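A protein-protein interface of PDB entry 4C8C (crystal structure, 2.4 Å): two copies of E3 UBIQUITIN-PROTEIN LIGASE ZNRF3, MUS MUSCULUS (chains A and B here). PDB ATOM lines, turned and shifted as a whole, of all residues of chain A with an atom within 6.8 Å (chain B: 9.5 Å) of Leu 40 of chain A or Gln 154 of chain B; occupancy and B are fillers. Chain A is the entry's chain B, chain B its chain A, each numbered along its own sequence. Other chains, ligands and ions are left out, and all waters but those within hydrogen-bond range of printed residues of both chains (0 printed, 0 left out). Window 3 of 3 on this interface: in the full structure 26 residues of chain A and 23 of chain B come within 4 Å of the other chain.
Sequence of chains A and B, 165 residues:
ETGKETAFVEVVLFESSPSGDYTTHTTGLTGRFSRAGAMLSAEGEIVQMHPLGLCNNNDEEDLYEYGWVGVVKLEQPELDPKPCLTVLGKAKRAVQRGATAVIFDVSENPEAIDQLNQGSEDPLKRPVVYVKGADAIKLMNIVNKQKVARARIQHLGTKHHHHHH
The side-chain hydroxyl of Ser 41 of chain A lies close to the side-chain hydroxyl of Ser 41 of chain B, 3.0 Å away.
The side-chain hydroxyl of Ser 41 of chain B sits at hydrogen-bond distance from the side-chain amide nitrogen of Gln 154 of chain A (3.1 Å).
OE1 of Glu 43 of chain B is in salt-bridge range of NH2 of Arg 126 of chain A, 3.6 Å away.
The backbone carbonyl oxygen of Phe 8 of chain B sits at hydrogen-bond distance from the backbone NH of Gln 154 of chain B, 2.9 Å away.
The side-chain carboxylate (OE1) of Glu 10 of chain B lies within salt-bridge range of the guanidinium group (NH1) of Arg 152 of chain B (3.1 Å).
The side-chain carboxylate (OE2) of Glu 43 of chain B is in salt-bridge range of the guanidinium group (NE) of Arg 152 of chain B (3.6 Å).
The backbone NH of Ala 38 of chain A is in hydrogen-bond range of the backbone carbonyl oxygen of Arg 126 of chain A, 3.1 Å away.
The side-chain hydroxyl (OG) of Ser 41 of chain A sits at hydrogen-bond distance from the backbone NH (N) of His 155 of chain A (3.1 Å).
O of Ala 42 of chain A lies within hydrogen-bond range of N of Ile 153 of chain A (2.6 Å).
CB of Leu 40 of chain A touches OE1 of Gln 154 of chain B, at 3.3 Å.
Ser 41 of chain A touches Gln 154 of chain B (N to OE1, 3.8 Å).
Ala 42 of chain A touches Glu 43 of chain B.
Arg 152 of chain B touches Arg 126 of chain A.
Leu 40 of chain A touches just one residue of chain B: Gln 154 (3.3 Å).
Gln 154 of chain B touches just these residues of chain A: Leu 40 (3.3 Å) and Ser 41 (3.8 Å).
No residue of chain B comes within 4 Å of Met 39 of chain A.
Of the printed residues of chain A, Glu 43 of chain B touches Ala 42 and Arg 126.
Printed residues of chain B within 4 Å of Ala 42 of chain A: Glu 43 (3.3 Å).
Gly 37 of chain A touches none of the printed residues of chain B.
Of the 26 printed residues of chain B, 4 touch a printed residue of chain A.
Hydrophobic or aromatic side chains of chain A within 4 Å of the printed part of chain B: Leu 40 and Ala 42.
Along chain A the printed residues that touch a printed residue of chain B span positions 40 to 154.
Among the printed residues, 7 pairs touch across the chains.
Leu 40 of chain A touches Gln 154 of chain B, but with the chains exchanged Gln 154 of chain A does not touch Leu 40 of chain B (4.5 Å).
Ser 41 of chain B touches its own counterpart, Ser 41 of chain A.
Ser 41 of chain A touches Gln 154 of chain B, and with the chains exchanged Gln 154 of chain A touches Ser 41 of chain B.
Positions printed for both chains: 33, 38, 39, 40, 41, 42, 101, 127, 129, 153, 154 and 155.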
ATOM      1  N   PHE A  33     -11.388  -9.043  15.711  1.00  0.00           N
ATOM      2  CA  PHE A  33     -11.292  -8.247  14.518  1.00  0.00           C
ATOM      3  C   PHE A  33     -12.495  -7.322  14.417  1.00  0.00           C
ATOM      4  O   PHE A  33     -13.575  -7.668  14.851  1.00  0.00           O
ATOM      5  CB  PHE A  33     -11.166  -9.163  13.294  1.00  0.00           C
ATOM      6  CG  PHE A  33      -9.843  -9.916  13.230  1.00  0.00           C
ATOM      7  CD1 PHE A  33      -8.677  -9.265  12.828  1.00  0.00           C
ATOM      8  CD2 PHE A  33      -9.754 -11.248  13.599  1.00  0.00           C
ATOM      9  CE1 PHE A  33      -7.469  -9.943  12.774  1.00  0.00           C
ATOM     10  CE2 PHE A  33      -8.547 -11.932  13.534  1.00  0.00           C
ATOM     11  CZ  PHE A  33      -7.401 -11.275  13.123  1.00  0.00           C
ATOM     12  N   GLY A  37     -11.891  -3.213   9.403  1.00  0.00           N
ATOM     13  CA  GLY A  37     -10.569  -3.546   8.866  1.00  0.00           C
ATOM     14  C   GLY A  37     -10.619  -4.920   8.247  1.00  0.00           C
ATOM     15  O   GLY A  37     -11.639  -5.565   8.309  1.00  0.00           O
ATOM     16  N   ALA A  38      -9.511  -5.375   7.673  1.00  0.00           N
ATOM     17  CA  ALA A  38      -9.450  -6.679   7.064  1.00  0.00           C
ATOM     18  C   ALA A  38      -9.333  -7.722   8.149  1.00  0.00           C
ATOM     19  O   ALA A  38      -8.828  -7.419   9.239  1.00  0.00           O
ATOM     20  CB  ALA A  38      -8.271  -6.767   6.130  1.00  0.00           C
ATOM     21  N   MET A  39      -9.844  -8.927   7.848  1.00  0.00           N
ATOM     22  CA  MET A  39      -9.703 -10.106   8.719  1.00  0.00           C
ATOM     23  C   MET A  39      -8.493 -10.916   8.195  1.00  0.00           C
ATOM     24  O   MET A  39      -8.642 -11.923   7.502  1.00  0.00           O
ATOM     25  CB  MET A  39     -11.012 -10.943   8.838  1.00  0.00           C
ATOM     26  N   LEU A  40      -7.285 -10.416   8.509  1.00  0.00           N
ATOM     27  CA  LEU A  40      -6.016 -11.066   8.150  1.00  0.00           C
ATOM     28  C   LEU A  40      -4.968 -11.021   9.264  1.00  0.00           C
ATOM     29  O   LEU A  40      -5.026 -10.221  10.204  1.00  0.00           O
ATOM     30  CB  LEU A  40      -5.369 -10.447   6.916  1.00  0.00           C
ATOM     31  CG  LEU A  40      -6.052  -9.691   5.776  1.00  0.00           C
ATOM     32  CD1 LEU A  40      -4.974  -8.938   4.993  1.00  0.00           C
ATOM     33  CD2 LEU A  40      -6.858 -10.583   4.827  1.00  0.00           C
ATOM     34  N   SER A  41      -3.983 -11.890   9.135  1.00  0.00           N
ATOM     35  CA  SER A  41      -2.912 -11.953  10.088  1.00  0.00           C
ATOM     36  C   SER A  41      -1.858 -10.865   9.795  1.00  0.00           C
ATOM     37  O   SER A  41      -1.803 -10.283   8.705  1.00  0.00           O
ATOM     38  CB  SER A  41      -2.267 -13.329  10.032  1.00  0.00           C
ATOM     39  OG  SER A  41      -3.152 -14.295  10.534  1.00  0.00           O
ATOM     40  N   ALA A  42      -1.022 -10.624  10.786  1.00  0.00           N
ATOM     41  CA  ALA A  42      -0.163  -9.502  10.742  1.00  0.00           C
ATOM     42  C   ALA A  42       0.762  -9.693  11.887  1.00  0.00           C
ATOM     43  O   ALA A  42       0.396 -10.282  12.906  1.00  0.00           O
ATOM     44  CB  ALA A  42      -0.958  -8.224  10.902  1.00  0.00           C
ATOM     45  N   ALA A 101      -0.776  -3.212  11.304  1.00  0.00           N
ATOM     46  CA  ALA A 101      -2.107  -3.558  11.889  1.00  0.00           C
ATOM     47  C   ALA A 101      -2.234  -2.606  13.079  1.00  0.00           C
ATOM     48  O   ALA A 101      -1.225  -2.127  13.542  1.00  0.00           O
ATOM     49  CB  ALA A 101      -2.150  -5.009  12.346  1.00  0.00           C
ATOM     50  N   LYS A 125      -7.500  -2.075   4.423  1.00  0.00           N
ATOM     51  CA  LYS A 125      -6.747  -3.222   3.910  1.00  0.00           C
ATOM     52  C   LYS A 125      -6.052  -4.064   5.017  1.00  0.00           C
ATOM     53  O   LYS A 125      -5.874  -5.292   4.892  1.00  0.00           O
ATOM     54  CB  LYS A 125      -5.728  -2.708   2.890  1.00  0.00           C
ATOM     55  CG  LYS A 125      -4.783  -1.665   3.486  1.00  0.00           C
ATOM     56  CD  LYS A 125      -4.117  -0.750   2.475  1.00  0.00           C
ATOM     57  CE  LYS A 125      -2.930  -0.073   3.156  1.00  0.00           C
ATOM     58  NZ  LYS A 125      -2.400   1.118   2.449  1.00  0.00           N
ATOM     59  N   ARG A 126      -5.666  -3.405   6.105  1.00  0.00           N
ATOM     60  CA  ARG A 126      -4.969  -4.063   7.211  1.00  0.00           C
ATOM     61  C   ARG A 126      -5.910  -4.345   8.318  1.00  0.00           C
ATOM     62  O   ARG A 126      -6.990  -3.751   8.366  1.00  0.00           O
ATOM     63  CB  ARG A 126      -3.868  -3.184   7.766  1.00  0.00           C
ATOM     64  CG  ARG A 126      -2.866  -2.727   6.724  1.00  0.00           C
ATOM     65  CD  ARG A 126      -2.297  -3.888   5.953  1.00  0.00           C
ATOM     66  NE  ARG A 126      -1.669  -4.821   6.848  1.00  0.00           N
ATOM     67  CZ  ARG A 126      -1.564  -6.135   6.633  1.00  0.00           C
ATOM     68  NH1 ARG A 126      -2.088  -6.736   5.542  1.00  0.00           N
ATOM     69  NH2 ARG A 126      -0.938  -6.884   7.532  1.00  0.00           N
ATOM     70  N   PRO A 127      -5.525  -5.277   9.215  1.00  0.00           N
ATOM     71  CA  PRO A 127      -6.310  -5.476  10.389  1.00  0.00           C
ATOM     72  C   PRO A 127      -6.344  -4.397  11.468  1.00  0.00           C
ATOM     73  O   PRO A 127      -5.307  -3.993  11.975  1.00  0.00           O
ATOM     74  CB  PRO A 127      -5.695  -6.749  10.998  1.00  0.00           C
ATOM     75  CG  PRO A 127      -4.517  -7.076  10.219  1.00  0.00           C
ATOM     76  CD  PRO A 127      -4.839  -6.530   8.880  1.00  0.00           C
ATOM     77  N   VAL A 129      -7.900  -4.505  15.303  1.00  0.00           N
ATOM     78  CA  VAL A 129      -8.304  -5.432  16.420  1.00  0.00           C
ATOM     79  C   VAL A 129      -8.567  -4.621  17.701  1.00  0.00           C
ATOM     80  O   VAL A 129      -7.832  -3.676  18.010  1.00  0.00           O
ATOM     81  CB  VAL A 129      -7.186  -6.455  16.783  1.00  0.00           C
ATOM     82  CG1 VAL A 129      -7.447  -7.127  18.123  1.00  0.00           C
ATOM     83  CG2 VAL A 129      -7.028  -7.534  15.721  1.00  0.00           C
ATOM     84  N   ILE A 153      -0.369 -11.237  15.146  1.00  0.00           N
ATOM     85  CA  ILE A 153      -1.832 -11.354  15.127  1.00  0.00           C
ATOM     86  C   ILE A 153      -2.257 -12.422  14.149  1.00  0.00           C
ATOM     87  O   ILE A 153      -1.863 -12.433  12.991  1.00  0.00           O
ATOM     88  CB  ILE A 153      -2.471 -10.054  14.681  1.00  0.00           C
ATOM     89  CG1 ILE A 153      -1.848  -8.870  15.439  1.00  0.00           C
ATOM     90  CG2 ILE A 153      -3.993 -10.078  14.889  1.00  0.00           C
ATOM     91  CD1 ILE A 153      -2.603  -7.584  15.174  1.00  0.00           C
ATOM     92  N   GLN A 154      -3.094 -13.319  14.643  1.00  0.00           N
ATOM     93  CA  GLN A 154      -3.497 -14.558  13.962  1.00  0.00           C
ATOM     94  C   GLN A 154      -5.013 -14.572  13.731  1.00  0.00           C
ATOM     95  O   GLN A 154      -5.768 -14.339  14.677  1.00  0.00           O
ATOM     96  CB  GLN A 154      -3.169 -15.699  14.908  1.00  0.00           C
ATOM     97  CG  GLN A 154      -2.507 -16.892  14.291  1.00  0.00           C
ATOM     98  CD  GLN A 154      -1.142 -16.525  13.795  1.00  0.00           C
ATOM     99  OE1 GLN A 154      -0.211 -16.335  14.582  1.00  0.00           O
ATOM    100  NE2 GLN A 154      -1.016 -16.400  12.483  1.00  0.00           N
ATOM    101  N   HIS A 155      -5.462 -14.829  12.500  1.00  0.00           N
ATOM    102  CA  HIS A 155      -6.877 -15.209  12.242  1.00  0.00           C
ATOM    103  C   HIS A 155      -7.028 -16.727  12.328  1.00  0.00           C
ATOM    104  O   HIS A 155      -6.459 -17.436  11.503  1.00  0.00           O
ATOM    105  CB  HIS A 155      -7.367 -14.740  10.860  1.00  0.00           C
ATOM    106  N   GLU B   5      -0.386 -27.647   2.370  1.00  0.00           N
ATOM    107  CA  GLU B   5      -1.238 -26.422   2.197  1.00  0.00           C
ATOM    108  C   GLU B   5      -0.448 -25.254   1.522  1.00  0.00           C
ATOM    109  O   GLU B   5       0.746 -25.018   1.787  1.00  0.00           O
ATOM    110  CB  GLU B   5      -1.855 -26.009   3.549  1.00  0.00           C
ATOM    111  N   THR B   6      -1.138 -24.540   0.640  1.00  0.00           N
ATOM    112  CA  THR B   6      -0.532 -23.498  -0.191  1.00  0.00           C
ATOM    113  C   THR B   6      -0.339 -22.224   0.643  1.00  0.00           C
ATOM    114  O   THR B   6      -1.191 -21.907   1.484  1.00  0.00           O
ATOM    115  CB  THR B   6      -1.388 -23.235  -1.469  1.00  0.00           C
ATOM    116  OG1 THR B   6      -0.719 -23.761  -2.634  1.00  0.00           O
ATOM    117  CG2 THR B   6      -1.675 -21.748  -1.693  1.00  0.00           C
ATOM    118  N   ALA B   7       0.772 -21.509   0.383  1.00  0.00           N
ATOM    119  CA  ALA B   7       1.116 -20.264   1.072  1.00  0.00           C
ATOM    120  C   ALA B   7       1.098 -19.063   0.136  1.00  0.00           C
ATOM    121  O   ALA B   7       1.815 -19.023  -0.857  1.00  0.00           O
ATOM    122  CB  ALA B   7       2.483 -20.392   1.716  1.00  0.00           C
ATOM    123  N   PHE B   8       0.280 -18.076   0.448  1.00  0.00           N
ATOM    124  CA  PHE B   8       0.267 -16.868  -0.344  1.00  0.00           C
ATOM    125  C   PHE B   8       1.330 -15.905   0.229  1.00  0.00           C
ATOM    126  O   PHE B   8       1.305 -15.556   1.414  1.00  0.00           O
ATOM    127  CB  PHE B   8      -1.151 -16.240  -0.400  1.00  0.00           C
ATOM    128  CG  PHE B   8      -1.214 -14.996  -1.266  1.00  0.00           C
ATOM    129  CD1 PHE B   8      -0.821 -15.053  -2.609  1.00  0.00           C
ATOM    130  CD2 PHE B   8      -1.614 -13.767  -0.732  1.00  0.00           C
ATOM    131  CE1 PHE B   8      -0.818 -13.927  -3.390  1.00  0.00           C
ATOM    132  CE2 PHE B   8      -1.594 -12.614  -1.512  1.00  0.00           C
ATOM    133  CZ  PHE B   8      -1.198 -12.698  -2.844  1.00  0.00           C
ATOM    134  N   VAL B   9       2.286 -15.533  -0.609  1.00  0.00           N
ATOM    135  CA  VAL B   9       3.331 -14.609  -0.210  1.00  0.00           C
ATOM    136  C   VAL B   9       3.172 -13.275  -0.881  1.00  0.00           C
ATOM    137  O   VAL B   9       3.041 -13.229  -2.089  1.00  0.00           O
ATOM    138  CB  VAL B   9       4.699 -15.113  -0.650  1.00  0.00           C
ATOM    139  CG1 VAL B   9       5.774 -14.141  -0.189  1.00  0.00           C
ATOM    140  CG2 VAL B   9       4.948 -16.525  -0.143  1.00  0.00           C
ATOM    141  N   GLU B  10       3.245 -12.205  -0.089  1.00  0.00           N
ATOM    142  CA  GLU B  10       3.283 -10.809  -0.571  1.00  0.00           C
ATOM    143  C   GLU B  10       4.607 -10.064  -0.268  1.00  0.00           C
ATOM    144  O   GLU B  10       5.091  -9.999   0.886  1.00  0.00           O
ATOM    145  CB  GLU B  10       2.152 -10.007   0.068  1.00  0.00           C
ATOM    146  CG  GLU B  10       0.891  -9.971  -0.774  1.00  0.00           C
ATOM    147  CD  GLU B  10      -0.281  -9.199  -0.156  1.00  0.00           C
ATOM    148  OE1 GLU B  10      -0.293  -8.890   1.078  1.00  0.00           O
ATOM    149  OE2 GLU B  10      -1.228  -8.927  -0.945  1.00  0.00           O
ATOM    150  N   LEU B  29       2.560 -13.941  -4.766  1.00  0.00           N
ATOM    151  CA  LEU B  29       3.325 -15.111  -5.073  1.00  0.00           C
ATOM    152  C   LEU B  29       2.654 -16.247  -4.369  1.00  0.00           C
ATOM    153  O   LEU B  29       2.060 -16.061  -3.302  1.00  0.00           O
ATOM    154  CB  LEU B  29       4.662 -15.042  -4.374  1.00  0.00           C
ATOM    155  CG  LEU B  29       5.990 -14.883  -5.052  1.00  0.00           C
ATOM    156  CD1 LEU B  29       6.385 -13.414  -5.085  1.00  0.00           C
ATOM    157  CD2 LEU B  29       6.938 -15.702  -4.193  1.00  0.00           C
ATOM    158  N   THR B  30       2.903 -17.433  -4.875  1.00  0.00           N
ATOM    159  CA  THR B  30       2.359 -18.636  -4.285  1.00  0.00           C
ATOM    160  C   THR B  30       3.466 -19.639  -4.099  1.00  0.00           C
ATOM    161  O   THR B  30       4.191 -19.946  -5.014  1.00  0.00           O
ATOM    162  CB  THR B  30       1.176 -19.183  -5.123  1.00  0.00           C
ATOM    163  OG1 THR B  30       0.005 -18.427  -4.774  1.00  0.00           O
ATOM    164  CG2 THR B  30       0.899 -20.652  -4.814  1.00  0.00           C
ATOM    165  N   GLY B  31       3.594 -20.119  -2.876  1.00  0.00           N
ATOM    166  CA  GLY B  31       4.511 -21.201  -2.547  1.00  0.00           C
ATOM    167  C   GLY B  31       3.790 -22.268  -1.745  1.00  0.00           C
ATOM    168  O   GLY B  31       2.556 -22.280  -1.719  1.00  0.00           O
ATOM    169  N   ARG B  32       4.557 -23.132  -1.068  1.00  0.00           N
ATOM    170  CA  ARG B  32       3.986 -24.206  -0.244  1.00  0.00           C
ATOM    171  C   ARG B  32       4.641 -24.221   1.154  1.00  0.00           C
ATOM    172  O   ARG B  32       5.822 -23.961   1.288  1.00  0.00           O
ATOM    173  CB  ARG B  32       4.153 -25.565  -0.976  1.00  0.00           C
ATOM    174  N   PHE B  33       3.861 -24.497   2.191  1.00  0.00           N
ATOM    175  CA  PHE B  33       4.417 -24.734   3.515  1.00  0.00           C
ATOM    176  C   PHE B  33       5.046 -26.095   3.642  1.00  0.00           C
ATOM    177  O   PHE B  33       4.433 -27.092   3.309  1.00  0.00           O
ATOM    178  CB  PHE B  33       3.327 -24.669   4.557  1.00  0.00           C
ATOM    179  CG  PHE B  33       2.806 -23.296   4.785  1.00  0.00           C
ATOM    180  CD1 PHE B  33       3.522 -22.406   5.537  1.00  0.00           C
ATOM    181  CD2 PHE B  33       1.609 -22.905   4.246  1.00  0.00           C
ATOM    182  CE1 PHE B  33       3.052 -21.137   5.736  1.00  0.00           C
ATOM    183  CE2 PHE B  33       1.116 -21.639   4.446  1.00  0.00           C
ATOM    184  CZ  PHE B  33       1.839 -20.752   5.199  1.00  0.00           C
ATOM    185  N   ALA B  38       5.866 -25.044  11.016  1.00  0.00           N
ATOM    186  CA  ALA B  38       4.483 -24.745  11.347  1.00  0.00           C
ATOM    187  C   ALA B  38       3.752 -24.212  10.137  1.00  0.00           C
ATOM    188  O   ALA B  38       4.377 -23.696   9.193  1.00  0.00           O
ATOM    189  CB  ALA B  38       4.384 -23.751  12.478  1.00  0.00           C
ATOM    190  N   MET B  39       2.428 -24.387  10.159  1.00  0.00           N
ATOM    191  CA  MET B  39       1.553 -23.885   9.110  1.00  0.00           C
ATOM    192  C   MET B  39       0.818 -22.689   9.719  1.00  0.00           C
ATOM    193  O   MET B  39      -0.346 -22.790  10.043  1.00  0.00           O
ATOM    194  CB  MET B  39       0.602 -24.991   8.568  1.00  0.00           C
ATOM    195  N   LEU B  40       1.568 -21.586   9.932  1.00  0.00           N
ATOM    196  CA  LEU B  40       1.066 -20.294  10.425  1.00  0.00           C
ATOM    197  C   LEU B  40       1.438 -19.203   9.450  1.00  0.00           C
ATOM    198  O   LEU B  40       2.355 -19.342   8.657  1.00  0.00           O
ATOM    199  CB  LEU B  40       1.688 -19.940  11.737  1.00  0.00           C
ATOM    200  CG  LEU B  40       1.553 -21.027  12.777  1.00  0.00           C
ATOM    201  CD1 LEU B  40       2.551 -20.756  13.885  1.00  0.00           C
ATOM    202  CD2 LEU B  40       0.113 -21.091  13.292  1.00  0.00           C
ATOM    203  N   SER B  41       0.710 -18.101   9.477  1.00  0.00           N
ATOM    204  CA  SER B  41       1.148 -16.930   8.727  1.00  0.00           C
ATOM    205  C   SER B  41       2.250 -16.169   9.540  1.00  0.00           C
ATOM    206  O   SER B  41       2.471 -16.436  10.728  1.00  0.00           O
ATOM    207  CB  SER B  41      -0.040 -16.052   8.370  1.00  0.00           C
ATOM    208  OG  SER B  41      -0.767 -15.723   9.510  1.00  0.00           O
ATOM    209  N   ALA B  42       3.005 -15.341   8.842  1.00  0.00           N
ATOM    210  CA  ALA B  42       4.130 -14.591   9.418  1.00  0.00           C
ATOM    211  C   ALA B  42       4.416 -13.496   8.421  1.00  0.00           C
ATOM    212  O   ALA B  42       4.107 -13.611   7.215  1.00  0.00           O
ATOM    213  CB  ALA B  42       5.346 -15.458   9.603  1.00  0.00           C
ATOM    214  N   GLU B  43       4.909 -12.404   8.935  1.00  0.00           N
ATOM    215  CA  GLU B  43       5.250 -11.254   8.122  1.00  0.00           C
ATOM    216  C   GLU B  43       6.456 -10.592   8.824  1.00  0.00           C
ATOM    217  O   GLU B  43       6.593 -10.769  10.009  1.00  0.00           O
ATOM    218  CB  GLU B  43       4.076 -10.293   8.119  1.00  0.00           C
ATOM    219  CG  GLU B  43       4.455  -8.813   8.210  1.00  0.00           C
ATOM    220  CD  GLU B  43       3.224  -7.946   8.248  1.00  0.00           C
ATOM    221  OE1 GLU B  43       2.143  -8.477   8.571  1.00  0.00           O
ATOM    222  OE2 GLU B  43       3.313  -6.740   7.974  1.00  0.00           O
ATOM    223  N   ALA B 101      10.218 -16.337   9.786  1.00  0.00           N
ATOM    224  CA  ALA B 101       9.865 -17.354   8.783  1.00  0.00           C
ATOM    225  C   ALA B 101      11.052 -17.483   7.870  1.00  0.00           C
ATOM    226  O   ALA B 101      11.881 -16.571   7.851  1.00  0.00           O
ATOM    227  CB  ALA B 101       8.632 -16.915   7.998  1.00  0.00           C
ATOM    228  N   ILE B 103      11.940 -18.729   3.671  1.00  0.00           N
ATOM    229  CA  ILE B 103      11.479 -19.038   2.330  1.00  0.00           C
ATOM    230  C   ILE B 103      12.702 -19.484   1.520  1.00  0.00           C
ATOM    231  O   ILE B 103      13.683 -18.731   1.368  1.00  0.00           O
ATOM    232  CB  ILE B 103      10.898 -17.802   1.650  1.00  0.00           C
ATOM    233  CG1 ILE B 103       9.853 -17.131   2.529  1.00  0.00           C
ATOM    234  CG2 ILE B 103      10.261 -18.142   0.305  1.00  0.00           C
ATOM    235  CD1 ILE B 103       9.077 -16.084   1.788  1.00  0.00           C
ATOM    236  N   PRO B 127       7.040 -20.836  10.318  1.00  0.00           N
ATOM    237  CA  PRO B 127       6.841 -21.376   8.971  1.00  0.00           C
ATOM    238  C   PRO B 127       8.120 -21.525   8.130  1.00  0.00           C
ATOM    239  O   PRO B 127       8.954 -20.597   8.091  1.00  0.00           O
ATOM    240  CB  PRO B 127       5.903 -20.368   8.296  1.00  0.00           C
ATOM    241  CG  PRO B 127       5.733 -19.228   9.222  1.00  0.00           C
ATOM    242  CD  PRO B 127       6.204 -19.647  10.576  1.00  0.00           C
ATOM    243  N   VAL B 129       8.758 -22.229   4.142  1.00  0.00           N
ATOM    244  CA  VAL B 129       8.026 -22.169   2.866  1.00  0.00           C
ATOM    245  C   VAL B 129       9.038 -22.395   1.744  1.00  0.00           C
ATOM    246  O   VAL B 129      10.188 -21.950   1.822  1.00  0.00           O
ATOM    247  CB  VAL B 129       7.281 -20.799   2.660  1.00  0.00           C
ATOM    248  CG1 VAL B 129       6.663 -20.680   1.263  1.00  0.00           C
ATOM    249  CG2 VAL B 129       6.188 -20.583   3.699  1.00  0.00           C
ATOM    250  N   ALA B 151       7.830  -8.937   3.725  1.00  0.00           N
ATOM    251  CA  ALA B 151       7.155 -10.092   3.220  1.00  0.00           C
ATOM    252  C   ALA B 151       6.001 -10.465   4.168  1.00  0.00           C
ATOM    253  O   ALA B 151       6.150 -10.383   5.388  1.00  0.00           O
ATOM    254  CB  ALA B 151       8.136 -11.238   3.100  1.00  0.00           C
ATOM    255  N   ARG B 152       4.852 -10.823   3.591  1.00  0.00           N
ATOM    256  CA  ARG B 152       3.757 -11.432   4.357  1.00  0.00           C
ATOM    257  C   ARG B 152       3.337 -12.791   3.793  1.00  0.00           C
ATOM    258  O   ARG B 152       3.023 -12.922   2.595  1.00  0.00           O
ATOM    259  CB  ARG B 152       2.554 -10.541   4.351  1.00  0.00           C
ATOM    260  CG  ARG B 152       2.866  -9.054   4.294  1.00  0.00           C
ATOM    261  CD  ARG B 152       1.594  -8.308   4.668  1.00  0.00           C
ATOM    262  NE  ARG B 152       1.724  -6.859   4.763  1.00  0.00           N
ATOM    263  CZ  ARG B 152       1.301  -5.994   3.833  1.00  0.00           C
ATOM    264  NH1 ARG B 152       0.723  -6.399   2.655  1.00  0.00           N
ATOM    265  NH2 ARG B 152       1.463  -4.696   4.074  1.00  0.00           N
ATOM    266  N   ILE B 153       3.315 -13.773   4.682  1.00  0.00           N
ATOM    267  CA  ILE B 153       3.032 -15.131   4.347  1.00  0.00           C
ATOM    268  C   ILE B 153       1.744 -15.497   5.031  1.00  0.00           C
ATOM    269  O   ILE B 153       1.681 -15.417   6.243  1.00  0.00           O
ATOM    270  CB  ILE B 153       4.148 -16.022   4.884  1.00  0.00           C
ATOM    271  CG1 ILE B 153       5.519 -15.417   4.542  1.00  0.00           C
ATOM    272  CG2 ILE B 153       4.085 -17.395   4.277  1.00  0.00           C
ATOM    273  CD1 ILE B 153       6.673 -16.325   4.930  1.00  0.00           C
ATOM    274  N   GLN B 154       0.742 -15.946   4.262  1.00  0.00           N
ATOM    275  CA  GLN B 154      -0.628 -16.232   4.775  1.00  0.00           C
ATOM    276  C   GLN B 154      -1.166 -17.677   4.638  1.00  0.00           C
ATOM    277  O   GLN B 154      -1.001 -18.310   3.587  1.00  0.00           O
ATOM    278  CB  GLN B 154      -1.607 -15.326   4.036  1.00  0.00           C
ATOM    279  CG  GLN B 154      -1.647 -13.896   4.543  1.00  0.00           C
ATOM    280  CD  GLN B 154      -2.781 -13.668   5.534  1.00  0.00           C
ATOM    281  OE1 GLN B 154      -3.498 -12.670   5.449  1.00  0.00           O
ATOM    282  NE2 GLN B 154      -2.967 -14.604   6.466  1.00  0.00           N
ATOM    283  N   HIS B 155      -1.826 -18.162   5.695  1.00  0.00           N
ATOM    284  CA  HIS B 155      -2.939 -19.184   5.613  1.00  0.00           C
ATOM    285  C   HIS B 155      -2.411 -20.588   5.706  1.00  0.00           C
ATOM    286  O   HIS B 155      -2.394 -21.171   6.790  1.00  0.00           O
ATOM    287  CB  HIS B 155      -3.815 -19.031   4.347  1.00  0.00           C
